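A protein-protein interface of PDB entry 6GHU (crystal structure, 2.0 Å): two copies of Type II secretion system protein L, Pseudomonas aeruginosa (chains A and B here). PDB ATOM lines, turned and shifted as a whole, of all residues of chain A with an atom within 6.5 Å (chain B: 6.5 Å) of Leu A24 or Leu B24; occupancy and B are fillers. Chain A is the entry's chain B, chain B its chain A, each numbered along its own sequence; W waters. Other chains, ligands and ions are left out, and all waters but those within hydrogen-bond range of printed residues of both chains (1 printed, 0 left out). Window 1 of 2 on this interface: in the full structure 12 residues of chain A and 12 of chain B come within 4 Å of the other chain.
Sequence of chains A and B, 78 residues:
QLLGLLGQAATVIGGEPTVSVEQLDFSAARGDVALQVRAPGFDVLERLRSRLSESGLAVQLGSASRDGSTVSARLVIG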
ATOM      1  N   LEU A   6      18.235 -17.581   7.260  1.00  0.00           N
ATOM      2  CA  LEU A   6      17.546 -17.557   8.545  1.00  0.00           C
ATOM      3  C   LEU A   6      17.591 -18.923   9.211  1.00  0.00           C
ATOM      4  O   LEU A   6      17.881 -19.035  10.408  1.00  0.00           O
ATOM      5  CB  LEU A   6      16.098 -17.110   8.352  1.00  0.00           C
ATOM      6  CG  LEU A   6      15.747 -15.728   8.893  1.00  0.00           C
ATOM      7  CD1 LEU A   6      14.323 -15.361   8.494  1.00  0.00           C
ATOM      8  CD2 LEU A   6      15.914 -15.681  10.411  1.00  0.00           C
ATOM      9  N   ILE A  13      22.628 -20.038  16.266  1.00  0.00           N
ATOM     10  CA  ILE A  13      22.249 -19.345  17.493  1.00  0.00           C
ATOM     11  C   ILE A  13      21.762 -20.348  18.527  1.00  0.00           C
ATOM     12  O   ILE A  13      22.036 -20.213  19.728  1.00  0.00           O
ATOM     13  CB  ILE A  13      21.191 -18.270  17.186  1.00  0.00           C
ATOM     14  CG1 ILE A  13      21.785 -17.215  16.249  1.00  0.00           C
ATOM     15  CG2 ILE A  13      20.697 -17.609  18.463  1.00  0.00           C
ATOM     16  CD1 ILE A  13      20.754 -16.381  15.508  1.00  0.00           C
ATOM     17  N   VAL A  21      17.116 -14.093  21.736  1.00  0.00           N
ATOM     18  CA  VAL A  21      16.725 -13.223  20.634  1.00  0.00           C
ATOM     19  C   VAL A  21      15.492 -12.450  21.077  1.00  0.00           C
ATOM     20  O   VAL A  21      14.390 -13.005  21.142  1.00  0.00           O
ATOM     21  CB  VAL A  21      16.446 -14.019  19.355  1.00  0.00           C
ATOM     22  CG1 VAL A  21      16.090 -13.076  18.212  1.00  0.00           C
ATOM     23  CG2 VAL A  21      17.644 -14.872  18.990  1.00  0.00           C
ATOM     24  N   GLU A  22      15.672 -11.163  21.376  1.00  0.00           N
ATOM     25  CA  GLU A  22      14.560 -10.342  21.835  1.00  0.00           C
ATOM     26  C   GLU A  22      13.709  -9.883  20.662  1.00  0.00           C
ATOM     27  O   GLU A  22      12.481  -9.805  20.770  1.00  0.00           O
ATOM     28  CB  GLU A  22      15.080  -9.129  22.606  1.00  0.00           C
ATOM     29  CG  GLU A  22      15.988  -9.473  23.783  1.00  0.00           C
ATOM     30  CD  GLU A  22      15.285 -10.318  24.827  1.00  0.00           C
ATOM     31  OE1 GLU A  22      15.731 -11.456  25.071  1.00  0.00           O
ATOM     32  OE2 GLU A  22      14.275  -9.844  25.392  1.00  0.00           O
ATOM     33  N   GLN A  23      14.349  -9.585  19.537  1.00  0.00           N
ATOM     34  CA  GLN A  23      13.656  -9.092  18.361  1.00  0.00           C
ATOM     35  C   GLN A  23      14.441  -9.512  17.129  1.00  0.00           C
ATOM     36  O   GLN A  23      15.671  -9.630  17.171  1.00  0.00           O
ATOM     37  CB  GLN A  23      13.496  -7.567  18.425  1.00  0.00           C
ATOM     38  CG  GLN A  23      12.818  -6.935  17.214  1.00  0.00           C
ATOM     39  CD  GLN A  23      13.786  -6.640  16.079  1.00  0.00           C
ATOM     40  OE1 GLN A  23      15.002  -6.778  16.228  1.00  0.00           O
ATOM     41  NE2 GLN A  23      13.246  -6.224  14.939  1.00  0.00           N
ATOM     42  N   LEU A  24      13.721  -9.742  16.037  1.00  0.00           N
ATOM     43  CA  LEU A  24      14.338 -10.094  14.770  1.00  0.00           C
ATOM     44  C   LEU A  24      13.462  -9.534  13.665  1.00  0.00           C
ATOM     45  O   LEU A  24      12.238  -9.682  13.712  1.00  0.00           O
ATOM     46  CB  LEU A  24      14.485 -11.610  14.629  1.00  0.00           C
ATOM     47  CG  LEU A  24      15.269 -12.136  13.427  1.00  0.00           C
ATOM     48  CD1 LEU A  24      15.863 -13.498  13.755  1.00  0.00           C
ATOM     49  CD2 LEU A  24      14.397 -12.246  12.192  1.00  0.00           C
ATOM     50  N   ASP A  25      14.077  -8.891  12.680  1.00  0.00           N
ATOM     51  CA  ASP A  25      13.309  -8.374  11.565  1.00  0.00           C
ATOM     52  C   ASP A  25      14.089  -8.564  10.278  1.00  0.00           C
ATOM     53  O   ASP A  25      15.321  -8.556  10.264  1.00  0.00           O
ATOM     54  CB  ASP A  25      12.922  -6.900  11.765  1.00  0.00           C
ATOM     55  CG  ASP A  25      14.097  -5.961  11.653  1.00  0.00           C
ATOM     56  OD1 ASP A  25      14.434  -5.581  10.511  1.00  0.00           O
ATOM     57  OD2 ASP A  25      14.665  -5.585  12.704  1.00  0.00           O
ATOM     58  N   PHE A  26      13.361  -8.933   9.234  1.00  0.00           N
ATOM     59  CA  PHE A  26      13.903  -8.961   7.891  1.00  0.00           C
ATOM     60  C   PHE A  26      12.999  -8.148   6.985  1.00  0.00           C
ATOM     61  O   PHE A  26      11.786  -8.056   7.197  1.00  0.00           O
ATOM     62  CB  PHE A  26      14.039 -10.375   7.311  1.00  0.00           C
ATOM     63  CG  PHE A  26      14.083 -10.389   5.807  1.00  0.00           C
ATOM     64  CD1 PHE A  26      15.197  -9.912   5.131  1.00  0.00           C
ATOM     65  CD2 PHE A  26      12.997 -10.830   5.070  1.00  0.00           C
ATOM     66  CE1 PHE A  26      15.234  -9.890   3.747  1.00  0.00           C
ATOM     67  CE2 PHE A  26      13.030 -10.817   3.682  1.00  0.00           C
ATOM     68  CZ  PHE A  26      14.150 -10.347   3.021  1.00  0.00           C
ATOM     69  N   SER A  27      13.620  -7.557   5.979  1.00  0.00           N
ATOM     70  CA  SER A  27      12.940  -6.791   4.943  1.00  0.00           C
ATOM     71  C   SER A  27      13.685  -6.966   3.628  1.00  0.00           C
ATOM     72  O   SER A  27      14.902  -6.765   3.570  1.00  0.00           O
ATOM     73  CB  SER A  27      12.864  -5.307   5.308  1.00  0.00           C
ATOM     74  OG  SER A  27      12.518  -4.533   4.177  1.00  0.00           O
ATOM     75  N   VAL A  33      19.171  -9.507   7.566  1.00  0.00           N
ATOM     76  CA  VAL A  33      18.406  -9.914   8.739  1.00  0.00           C
ATOM     77  C   VAL A  33      19.045  -9.261   9.959  1.00  0.00           C
ATOM     78  O   VAL A  33      20.245  -9.443  10.205  1.00  0.00           O
ATOM     79  CB  VAL A  33      18.368 -11.445   8.885  1.00  0.00           C
ATOM     80  CG1 VAL A  33      17.522 -11.853  10.089  1.00  0.00           C
ATOM     81  CG2 VAL A  33      17.833 -12.091   7.608  1.00  0.00           C
ATOM     82  N   ALA A  34      18.249  -8.513  10.721  1.00  0.00           N
ATOM     83  CA  ALA A  34      18.718  -7.835  11.925  1.00  0.00           C
ATOM     84  C   ALA A  34      18.143  -8.508  13.165  1.00  0.00           C
ATOM     85  O   ALA A  34      16.953  -8.834  13.214  1.00  0.00           O
ATOM     86  CB  ALA A  34      18.331  -6.356  11.925  1.00  0.00           C
ATOM     87  N   LEU A  35      18.996  -8.692  14.172  1.00  0.00           N
ATOM     88  CA  LEU A  35      18.655  -9.409  15.392  1.00  0.00           C
ATOM     89  C   LEU A  35      19.093  -8.598  16.602  1.00  0.00           C
ATOM     90  O   LEU A  35      20.254  -8.185  16.688  1.00  0.00           O
ATOM     91  CB  LEU A  35      19.332 -10.789  15.445  1.00  0.00           C
ATOM     92  CG  LEU A  35      18.924 -11.871  14.447  1.00  0.00           C
ATOM     93  CD1 LEU A  35      19.643 -11.694  13.122  1.00  0.00           C
ATOM     94  CD2 LEU A  35      19.205 -13.252  15.031  1.00  0.00           C
ATOM     95  N   GLN A  36      18.166  -8.379  17.532  1.00  0.00           N
ATOM     96  CA  GLN A  36      18.488  -7.843  18.850  1.00  0.00           C
ATOM     97  C   GLN A  36      18.678  -9.016  19.803  1.00  0.00           C
ATOM     98  O   GLN A  36      17.729  -9.764  20.065  1.00  0.00           O
ATOM     99  CB  GLN A  36      17.376  -6.925  19.355  1.00  0.00           C
ATOM    100  CG  GLN A  36      17.163  -5.676  18.523  1.00  0.00           C
ATOM    101  CD  GLN A  36      18.220  -4.632  18.761  1.00  0.00           C
ATOM    102  OE1 GLN A  36      19.057  -4.766  19.659  1.00  0.00           O
ATOM    103  NE2 GLN A  36      18.187  -3.571  17.963  1.00  0.00           N
ATOM    104  N   LEU B   6      11.670 -20.797  13.846  1.00  0.00           N
ATOM    105  CA  LEU B   6      12.224 -20.109  12.687  1.00  0.00           C
ATOM    106  C   LEU B   6      12.771 -21.097  11.670  1.00  0.00           C
ATOM    107  O   LEU B   6      12.371 -21.102  10.500  1.00  0.00           O
ATOM    108  CB  LEU B   6      13.340 -19.168  13.126  1.00  0.00           C
ATOM    109  CG  LEU B   6      13.034 -17.718  13.464  1.00  0.00           C
ATOM    110  CD1 LEU B   6      14.385 -17.029  13.617  1.00  0.00           C
ATOM    111  CD2 LEU B   6      12.164 -17.040  12.405  1.00  0.00           C
ATOM    112  N   ILE B  13       8.672 -23.194   4.199  1.00  0.00           N
ATOM    113  CA  ILE B  13       8.392 -22.178   3.187  1.00  0.00           C
ATOM    114  C   ILE B  13       9.284 -22.384   1.973  1.00  0.00           C
ATOM    115  O   ILE B  13       8.882 -22.095   0.838  1.00  0.00           O
ATOM    116  CB  ILE B  13       8.547 -20.770   3.791  1.00  0.00           C
ATOM    117  CG1 ILE B  13       7.543 -20.585   4.927  1.00  0.00           C
ATOM    118  CG2 ILE B  13       8.313 -19.695   2.738  1.00  0.00           C
ATOM    119  CD1 ILE B  13       7.886 -19.473   5.883  1.00  0.00           C
ATOM    120  N   VAL B  21       8.850 -14.189   0.701  1.00  0.00           N
ATOM    121  CA  VAL B  21       8.744 -13.563   2.014  1.00  0.00           C
ATOM    122  C   VAL B  21       9.246 -12.135   1.875  1.00  0.00           C
ATOM    123  O   VAL B  21      10.453 -11.899   1.760  1.00  0.00           O
ATOM    124  CB  VAL B  21       9.539 -14.330   3.078  1.00  0.00           C
ATOM    125  CG1 VAL B  21       9.365 -13.670   4.436  1.00  0.00           C
ATOM    126  CG2 VAL B  21       9.094 -15.778   3.132  1.00  0.00           C
ATOM    127  N   GLU B  22       8.320 -11.181   1.890  1.00  0.00           N
ATOM    128  CA  GLU B  22       8.683  -9.781   1.713  1.00  0.00           C
ATOM    129  C   GLU B  22       9.226  -9.190   3.002  1.00  0.00           C
ATOM    130  O   GLU B  22      10.150  -8.372   2.975  1.00  0.00           O
ATOM    131  CB  GLU B  22       7.467  -8.976   1.252  1.00  0.00           C
ATOM    132  CG  GLU B  22       6.750  -9.542   0.029  1.00  0.00           C
ATOM    133  CD  GLU B  22       7.598  -9.471  -1.222  1.00  0.00           C
ATOM    134  OE1 GLU B  22       7.562 -10.431  -2.023  1.00  0.00           O
ATOM    135  OE2 GLU B  22       8.304  -8.456  -1.402  1.00  0.00           O
ATOM    136  N   GLN B  23       8.655  -9.582   4.137  1.00  0.00           N
ATOM    137  CA  GLN B  23       9.052  -9.060   5.434  1.00  0.00           C
ATOM    138  C   GLN B  23       8.771 -10.132   6.473  1.00  0.00           C
ATOM    139  O   GLN B  23       7.897 -10.983   6.288  1.00  0.00           O
ATOM    140  CB  GLN B  23       8.297  -7.765   5.780  1.00  0.00           C
ATOM    141  CG  GLN B  23       9.107  -6.721   6.561  1.00  0.00           C
ATOM    142  CD  GLN B  23       9.045  -6.897   8.077  1.00  0.00           C
ATOM    143  OE1 GLN B  23       8.311  -7.743   8.590  1.00  0.00           O
ATOM    144  NE2 GLN B  23       9.814  -6.085   8.799  1.00  0.00           N
ATOM    145  N   LEU B  24       9.523 -10.088   7.566  1.00  0.00           N
ATOM    146  CA  LEU B  24       9.326 -11.024   8.660  1.00  0.00           C
ATOM    147  C   LEU B  24       9.806 -10.356   9.934  1.00  0.00           C
ATOM    148  O   LEU B  24      10.796  -9.619   9.914  1.00  0.00           O
ATOM    149  CB  LEU B  24      10.071 -12.341   8.410  1.00  0.00           C
ATOM    150  CG  LEU B  24      10.187 -13.335   9.575  1.00  0.00           C
ATOM    151  CD1 LEU B  24      10.287 -14.755   9.047  1.00  0.00           C
ATOM    152  CD2 LEU B  24      11.399 -13.044  10.459  1.00  0.00           C
ATOM    153  N   ASP B  25       9.105 -10.611  11.034  1.00  0.00           N
ATOM    154  CA  ASP B  25       9.513 -10.015  12.294  1.00  0.00           C
ATOM    155  C   ASP B  25       8.956 -10.817  13.457  1.00  0.00           C
ATOM    156  O   ASP B  25       7.870 -11.396  13.373  1.00  0.00           O
ATOM    157  CB  ASP B  25       9.055  -8.554  12.395  1.00  0.00           C
ATOM    158  CG  ASP B  25       7.555  -8.415  12.616  1.00  0.00           C
ATOM    159  OD1 ASP B  25       7.115  -8.484  13.783  1.00  0.00           O
ATOM    160  OD2 ASP B  25       6.815  -8.219  11.626  1.00  0.00           O
ATOM    161  N   PHE B  26       9.732 -10.835  14.540  1.00  0.00           N
ATOM    162  CA  PHE B  26       9.329 -11.406  15.815  1.00  0.00           C
ATOM    163  C   PHE B  26       9.767 -10.464  16.927  1.00  0.00           C
ATOM    164  O   PHE B  26      10.751  -9.733  16.787  1.00  0.00           O
ATOM    165  CB  PHE B  26       9.941 -12.801  16.022  1.00  0.00           C
ATOM    166  CG  PHE B  26      10.213 -13.139  17.463  1.00  0.00           C
ATOM    167  CD1 PHE B  26       9.229 -13.710  18.253  1.00  0.00           C
ATOM    168  CD2 PHE B  26      11.455 -12.887  18.024  1.00  0.00           C
ATOM    169  CE1 PHE B  26       9.476 -14.020  19.575  1.00  0.00           C
ATOM    170  CE2 PHE B  26      11.707 -13.190  19.349  1.00  0.00           C
ATOM    171  CZ  PHE B  26      10.718 -13.758  20.125  1.00  0.00           C
ATOM    172  N   SER B  27       9.018 -10.472  18.028  1.00  0.00           N
ATOM    173  CA  SER B  27       9.464  -9.851  19.264  1.00  0.00           C
ATOM    174  C   SER B  27       9.079 -10.775  20.405  1.00  0.00           C
ATOM    175  O   SER B  27       7.995 -11.366  20.395  1.00  0.00           O
ATOM    176  CB  SER B  27       8.840  -8.466  19.478  1.00  0.00           C
ATOM    177  OG  SER B  27       7.535  -8.576  20.020  1.00  0.00           O
ATOM    178  N   VAL B  33       5.851 -15.072  15.443  1.00  0.00           N
ATOM    179  CA  VAL B  33       6.561 -14.649  14.243  1.00  0.00           C
ATOM    180  C   VAL B  33       5.531 -14.247  13.196  1.00  0.00           C
ATOM    181  O   VAL B  33       4.629 -15.029  12.873  1.00  0.00           O
ATOM    182  CB  VAL B  33       7.470 -15.769  13.707  1.00  0.00           C
ATOM    183  CG1 VAL B  33       8.312 -15.263  12.545  1.00  0.00           C
ATOM    184  CG2 VAL B  33       8.352 -16.330  14.814  1.00  0.00           C
ATOM    185  N   ALA B  34       5.677 -13.040  12.654  1.00  0.00           N
ATOM    186  CA  ALA B  34       4.791 -12.531  11.616  1.00  0.00           C
ATOM    187  C   ALA B  34       5.551 -12.429  10.302  1.00  0.00           C
ATOM    188  O   ALA B  34       6.669 -11.905  10.269  1.00  0.00           O
ATOM    189  CB  ALA B  34       4.228 -11.161  11.998  1.00  0.00           C
ATOM    190  N   LEU B  35       4.938 -12.920   9.225  1.00  0.00           N
ATOM    191  CA  LEU B  35       5.530 -12.902   7.893  1.00  0.00           C
ATOM    192  C   LEU B  35       4.556 -12.263   6.916  1.00  0.00           C
ATOM    193  O   LEU B  35       3.369 -12.602   6.909  1.00  0.00           O
ATOM    194  CB  LEU B  35       5.871 -14.316   7.396  1.00  0.00           C
ATOM    195  CG  LEU B  35       6.689 -15.264   8.272  1.00  0.00           C
ATOM    196  CD1 LEU B  35       5.827 -15.918   9.340  1.00  0.00           C
ATOM    197  CD2 LEU B  35       7.349 -16.326   7.392  1.00  0.00           C
ATOM    198  N   GLN B  36       5.061 -11.352   6.090  1.00  0.00           N
ATOM    199  CA  GLN B  36       4.334 -10.840   4.935  1.00  0.00           C
ATOM    200  C   GLN B  36       4.792 -11.640   3.728  1.00  0.00           C
ATOM    201  O   GLN B  36       5.976 -11.604   3.373  1.00  0.00           O
ATOM    202  CB  GLN B  36       4.596  -9.350   4.723  1.00  0.00           C
ATOM    203  CG  GLN B  36       4.117  -8.458   5.854  1.00  0.00           C
ATOM    204  CD  GLN B  36       2.612  -8.317   5.885  1.00  0.00           C
ATOM    205  OE1 GLN B  36       1.915  -8.758   4.969  1.00  0.00           O
ATOM    206  NE2 GLN B  36       2.098  -7.688   6.937  1.00  0.00           N
HETATM  207  O   HOH W   1      12.558  -5.086   8.441  1.00  0.00           O
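CD2 of Leu A6 touches CD1 of Leu B6 (3.8 Å). Glu A22 touches Phe B26 (O to CE2, 3.8 Å). Ser B27 touches Glu A22. Leu A24 touches Leu B6 (CD1 to CD1, 3.8 Å). CD2 of Leu A24 touches CD2 of Leu B24 (3.6 Å). CA of Asp B25 touches O of Leu A24, 3.1 Å away. Asp A25 touches Leu B24. CE2 of Phe A26 touches O of Val B21 (3.4 Å). CE2 of Phe A26 touches O of Glu B22 (3.8 Å). Glu B22 touches Ser A27.
Gln A23 touches Phe B26, and with the chains exchanged Phe A26 touches Gln B23. Leu A24 touches its own counterpart, Leu B24. Leu A24 touches Asp B25, and with the chains exchanged Asp A25 touches Leu B24. Leu A24 touches Phe B26, and with the chains exchanged Phe A26 touches Leu B24. Positions printed for both chains: 6, 13, 21, 22, 23, 24, 25, 26, 27, 33, 34, 35 and 36. Of the 15 pairs that touch across the chains among the printed residues, 14 have their exchanged pair printed and touching as well.
The side-chain carboxylate of Asp B25 lies close to the side-chain amide oxygen of Gln B23, 3.4 Å away. The backbone NH of Asp A25 lies within hydrogen-bond range of the backbone carbonyl oxygen of Ala A34 (2.9 Å). The backbone NH (N) of Glu B22 is in hydrogen-bond range of the backbone carbonyl oxygen (O) of Gln B36, at 2.8 Å. O of Gln A23 is in hydrogen-bond range of N of Gln A36 (2.8 Å). The backbone carbonyl oxygen of Gln B23 sits at hydrogen-bond distance from the backbone NH of Gln B36 (2.9 Å). The backbone carbonyl oxygen (O) of Gln A36 is in hydrogen-bond range of the backbone NH (N) of Glu A22.
Of the 13 printed residues of chain A, 8 touch a printed residue of chain B. Printed residues of chain A that touch a printed residue of chain B: Leu A6, Val A21, Glu A22, Gln A23, Leu A24, Asp A25, Phe A26 and Ser A27. Among the printed residues, 15 pairs touch across the chains. Among the printed residues, no Asp or Glu carboxylate lies within 4 Å of a Lys or Arg side-chain nitrogen of the other chain.
Water W1 lies within hydrogen-bond range of OD1 of Asp A25, NE2 of Gln B23 and O of Phe A26.
Printed residues of chain B within 4 Å of Leu A24: Leu B6, Leu B24, Asp B25 and Phe B26. Of the printed residues of chain A, Leu B24 touches Leu A24 (3.6 Å), Asp A25 (3.3 Å) and Phe A26 (2.7 Å). Printed residues of chain B within 4 Å of Ser A27: Glu B22 (3.8 Å). Of the printed residues of chain B, Val A21 touches Phe B26 (3.2 Å). Printed residues of chain B within 4 Å of Asp A25: Leu B24 (3.3 Å). Of the printed residues of chain B, Leu A6 touches Leu B6 (3.8 Å). Ala A34 touches none of the printed residues of chain B. Gln A36 touches none of the printed residues of chain B. The nearest printed residue of chain B that does not touch Leu A24 is Ser B27 (5.2 Å). The nearest printed residue of chain A that does not touch Leu B24 is Leu A6 (4.1 Å). The nearest printed residue of chain A that does not touch Val B21 is Ser A27 (6.2 Å).
The backbone carbonyl oxygen (O) of Phe A26 lies close to the side-chain amide nitrogen (NE2) of Gln B23, at 3.2 Å. N of Phe B26 sits at hydrogen-bond distance from O of Leu A24 (2.9 Å). O of Leu B24 lies within hydrogen-bond range of N of Phe A26 (2.7 Å).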
